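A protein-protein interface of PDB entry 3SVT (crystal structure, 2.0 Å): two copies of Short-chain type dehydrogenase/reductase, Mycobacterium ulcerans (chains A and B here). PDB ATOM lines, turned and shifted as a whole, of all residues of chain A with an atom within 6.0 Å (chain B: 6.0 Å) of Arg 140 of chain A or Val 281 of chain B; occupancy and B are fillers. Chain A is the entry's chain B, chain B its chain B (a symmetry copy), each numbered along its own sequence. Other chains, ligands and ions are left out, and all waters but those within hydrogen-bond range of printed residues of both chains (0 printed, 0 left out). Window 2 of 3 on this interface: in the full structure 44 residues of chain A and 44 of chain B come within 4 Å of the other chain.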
ATOM      1  N   ALA A 135      35.205  12.899 -20.644  1.00  0.00           N
ATOM      2  CA  ALA A 135      34.346  13.572 -21.601  1.00  0.00           C
ATOM      3  C   ALA A 135      32.910  13.682 -21.098  1.00  0.00           C
ATOM      4  O   ALA A 135      32.289  14.730 -21.257  1.00  0.00           O
ATOM      5  CB  ALA A 135      34.379  12.864 -22.943  1.00  0.00           C
ATOM      6  N   ARG A 136      32.372  12.612 -20.515  1.00  0.00           N
ATOM      7  CA  ARG A 136      30.993  12.668 -20.009  1.00  0.00           C
ATOM      8  C   ARG A 136      30.804  13.869 -19.062  1.00  0.00           C
ATOM      9  O   ARG A 136      29.851  14.617 -19.192  1.00  0.00           O
ATOM     10  CB  ARG A 136      30.619  11.390 -19.269  1.00  0.00           C
ATOM     11  CG  ARG A 136      30.454  10.158 -20.150  1.00  0.00           C
ATOM     12  CD  ARG A 136      30.207   8.909 -19.264  1.00  0.00           C
ATOM     13  NE  ARG A 136      29.925   7.725 -20.066  1.00  0.00           N
ATOM     14  CZ  ARG A 136      29.558   6.533 -19.587  1.00  0.00           C
ATOM     15  NH1 ARG A 136      29.429   6.310 -18.283  1.00  0.00           N
ATOM     16  NH2 ARG A 136      29.329   5.546 -20.426  1.00  0.00           N
ATOM     17  N   GLU A 137      31.730  14.046 -18.113  1.00  0.00           N
ATOM     18  CA  GLU A 137      31.586  15.114 -17.122  1.00  0.00           C
ATOM     19  C   GLU A 137      31.856  16.475 -17.713  1.00  0.00           C
ATOM     20  O   GLU A 137      31.157  17.438 -17.385  1.00  0.00           O
ATOM     21  CB  GLU A 137      32.496  14.904 -15.919  1.00  0.00           C
ATOM     22  CG  GLU A 137      32.296  13.574 -15.188  1.00  0.00           C
ATOM     23  CD  GLU A 137      30.885  13.371 -14.692  1.00  0.00           C
ATOM     24  OE1 GLU A 137      30.186  14.365 -14.439  1.00  0.00           O
ATOM     25  OE2 GLU A 137      30.475  12.203 -14.578  1.00  0.00           O
ATOM     26  N   MET A 138      32.859  16.568 -18.579  1.00  0.00           N
ATOM     27  CA  MET A 138      33.167  17.857 -19.205  1.00  0.00           C
ATOM     28  C   MET A 138      32.011  18.336 -20.082  1.00  0.00           C
ATOM     29  O   MET A 138      31.708  19.535 -20.104  1.00  0.00           O
ATOM     30  CB  MET A 138      34.495  17.825 -19.986  1.00  0.00           C
ATOM     31  CG  MET A 138      35.706  18.093 -19.104  1.00  0.00           C
ATOM     32  SD  MET A 138      37.326  17.908 -19.914  1.00  0.00           S
ATOM     33  CE  MET A 138      37.143  16.252 -20.551  1.00  0.00           C
ATOM     34  N   VAL A 139      31.345  17.418 -20.779  1.00  0.00           N
ATOM     35  CA  VAL A 139      30.149  17.782 -21.527  1.00  0.00           C
ATOM     36  C   VAL A 139      29.044  18.281 -20.579  1.00  0.00           C
ATOM     37  O   VAL A 139      28.477  19.353 -20.781  1.00  0.00           O
ATOM     38  CB  VAL A 139      29.624  16.603 -22.394  1.00  0.00           C
ATOM     39  CG1 VAL A 139      28.259  16.938 -22.988  1.00  0.00           C
ATOM     40  CG2 VAL A 139      30.623  16.260 -23.526  1.00  0.00           C
ATOM     41  N   ARG A 140      28.744  17.512 -19.540  1.00  0.00           N
ATOM     42  CA  ARG A 140      27.757  17.953 -18.534  1.00  0.00           C
ATOM     43  C   ARG A 140      28.112  19.293 -17.882  1.00  0.00           C
ATOM     44  O   ARG A 140      27.229  20.075 -17.541  1.00  0.00           O
ATOM     45  CB  ARG A 140      27.589  16.909 -17.424  1.00  0.00           C
ATOM     46  CG  ARG A 140      27.232  15.527 -17.915  1.00  0.00           C
ATOM     47  CD  ARG A 140      26.224  14.821 -17.035  1.00  0.00           C
ATOM     48  NE  ARG A 140      26.348  13.368 -17.184  1.00  0.00           N
ATOM     49  CZ  ARG A 140      26.975  12.554 -16.326  1.00  0.00           C
ATOM     50  NH1 ARG A 140      27.035  11.254 -16.591  1.00  0.00           N
ATOM     51  NH2 ARG A 140      27.541  13.014 -15.214  1.00  0.00           N
ATOM     52  N   GLY A 141      29.403  19.551 -17.694  1.00  0.00           N
ATOM     53  CA  GLY A 141      29.855  20.804 -17.094  1.00  0.00           C
ATOM     54  C   GLY A 141      29.818  22.019 -18.000  1.00  0.00           C
ATOM     55  O   GLY A 141      30.098  23.121 -17.543  1.00  0.00           O
ATOM     56  N   GLY A 142      29.484  21.842 -19.275  1.00  0.00           N
ATOM     57  CA  GLY A 142      29.384  22.964 -20.202  1.00  0.00           C
ATOM     58  C   GLY A 142      30.645  23.237 -21.013  1.00  0.00           C
ATOM     59  O   GLY A 142      30.753  24.269 -21.681  1.00  0.00           O
ATOM     60  N   GLY A 143      31.606  22.312 -20.969  1.00  0.00           N
ATOM     61  CA  GLY A 143      32.827  22.445 -21.738  1.00  0.00           C
ATOM     62  C   GLY A 143      34.075  22.133 -20.945  1.00  0.00           C
ATOM     63  O   GLY A 143      34.040  21.971 -19.724  1.00  0.00           O
ATOM     64  N   THR B 109      31.476   8.702 -25.791  1.00  0.00           N
ATOM     65  CA  THR B 109      31.052   8.681 -24.392  1.00  0.00           C
ATOM     66  C   THR B 109      30.214   7.448 -23.975  1.00  0.00           C
ATOM     67  O   THR B 109      30.071   7.171 -22.776  1.00  0.00           O
ATOM     68  CB  THR B 109      30.252   9.970 -24.044  1.00  0.00           C
ATOM     69  OG1 THR B 109      29.282  10.195 -25.057  1.00  0.00           O
ATOM     70  CG2 THR B 109      31.169  11.196 -24.008  1.00  0.00           C
ATOM     71  N   GLN B 110      29.641   6.726 -24.930  1.00  0.00           N
ATOM     72  CA  GLN B 110      28.835   5.541 -24.595  1.00  0.00           C
ATOM     73  C   GLN B 110      29.369   4.278 -25.226  1.00  0.00           C
ATOM     74  O   GLN B 110      28.696   3.244 -25.238  1.00  0.00           O
ATOM     75  CB  GLN B 110      27.379   5.745 -25.035  1.00  0.00           C
ATOM     76  CG  GLN B 110      26.639   6.873 -24.289  1.00  0.00           C
ATOM     77  CD  GLN B 110      26.125   6.439 -22.923  1.00  0.00           C
ATOM     78  OE1 GLN B 110      26.843   5.782 -22.165  1.00  0.00           O
ATOM     79  NE2 GLN B 110      24.868   6.783 -22.607  1.00  0.00           N
ATOM     80  N   ALA B 276      23.106  13.010 -27.039  1.00  0.00           N
ATOM     81  CA  ALA B 276      24.043  11.898 -26.921  1.00  0.00           C
ATOM     82  C   ALA B 276      25.134  11.934 -27.998  1.00  0.00           C
ATOM     83  O   ALA B 276      26.235  11.471 -27.764  1.00  0.00           O
ATOM     84  CB  ALA B 276      23.295  10.546 -26.959  1.00  0.00           C
ATOM     85  N   GLY B 279      28.045  13.841 -26.910  1.00  0.00           N
ATOM     86  CA  GLY B 279      28.385  13.445 -25.572  1.00  0.00           C
ATOM     87  C   GLY B 279      27.180  13.834 -24.757  1.00  0.00           C
ATOM     88  O   GLY B 279      26.197  14.310 -25.290  1.00  0.00           O
ATOM     89  N   LEU B 280      27.213  13.684 -23.472  1.00  0.00           N
ATOM     90  CA  LEU B 280      25.976  13.950 -22.722  1.00  0.00           C
ATOM     91  C   LEU B 280      25.240  12.633 -22.580  1.00  0.00           C
ATOM     92  O   LEU B 280      24.519  12.183 -23.467  1.00  0.00           O
ATOM     93  CB  LEU B 280      25.072  15.037 -23.345  1.00  0.00           C
ATOM     94  CG  LEU B 280      23.998  15.527 -22.354  1.00  0.00           C
ATOM     95  CD1 LEU B 280      24.566  15.736 -20.956  1.00  0.00           C
ATOM     96  CD2 LEU B 280      23.337  16.816 -22.814  1.00  0.00           C
ATOM     97  N   VAL B 281      25.489  12.036 -21.421  1.00  0.00           N
ATOM     98  CA  VAL B 281      24.988  10.741 -21.009  1.00  0.00           C
ATOM     99  C   VAL B 281      23.896  10.970 -19.975  1.00  0.00           C
ATOM    100  O   VAL B 281      24.074  11.801 -19.091  1.00  0.00           O
ATOM    101  CB  VAL B 281      26.114   9.907 -20.356  1.00  0.00           C
ATOM    102  OXT VAL B 281      22.808  10.364 -19.992  1.00  0.00           O
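Of the 9 printed residues of chain A, 4 touch a printed residue of chain B.
Along chain A the printed residues that touch a printed residue of chain B span positions 135 to 140.
Hydrophobic or aromatic side chains of chain B within 4 Å of the printed part of chain A: Leu 280.
Along chain B the printed residues that touch a printed residue of chain A span positions 109 to 281.
NH2 of Arg 140 of chain A is in salt-bridge range of OE1 of Glu 137 of chain A (3.1 Å).
The guanidinium group (NE) of Arg 136 of chain A lies within hydrogen-bond range of the backbone carbonyl oxygen (O) of Thr 109 of chain B (2.8 Å).
The guanidinium group (NH2) of Arg 136 of chain A is in hydrogen-bond range of the side-chain amide oxygen (OE1) of Gln 110 of chain B (3.0 Å).
The guanidinium group of Arg 140 of chain A is in salt-bridge range of the chain-end carboxylate of Val 281 of chain B (3.4 Å).
Ala 135 of chain A touches Thr 109 of chain B (CB to CG2, 3.8 Å).
Gly 279 of chain B touches Val 139 of chain A.
Leu 280 of chain B touches Val 139 of chain A (N to CG1, 3.5 Å).
Arg 140 of chain A touches one residue of chain B.
Of chain A, only Arg 140 (3.4 Å) comes within 4 Å of Val 281 of chain B.
Of the printed residues of chain B, Val 139 of chain A touches Gly 279 (3.7 Å) and Leu 280 (3.5 Å).
Of the printed residues of chain A, Gln 110 of chain B touches Arg 136 (3.0 Å).
Of the printed residues of chain A, Gly 279 of chain B touches Val 139 (3.7 Å).
Gly 142 of chain A touches none of the printed residues of chain B.
Glu 137 of chain A touches none of the printed residues of chain B.
The nearest residue of chain B that does not touch Arg 140 of chain A is Leu 280 of chain B (4.05 Å).
No position is printed for both chains.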
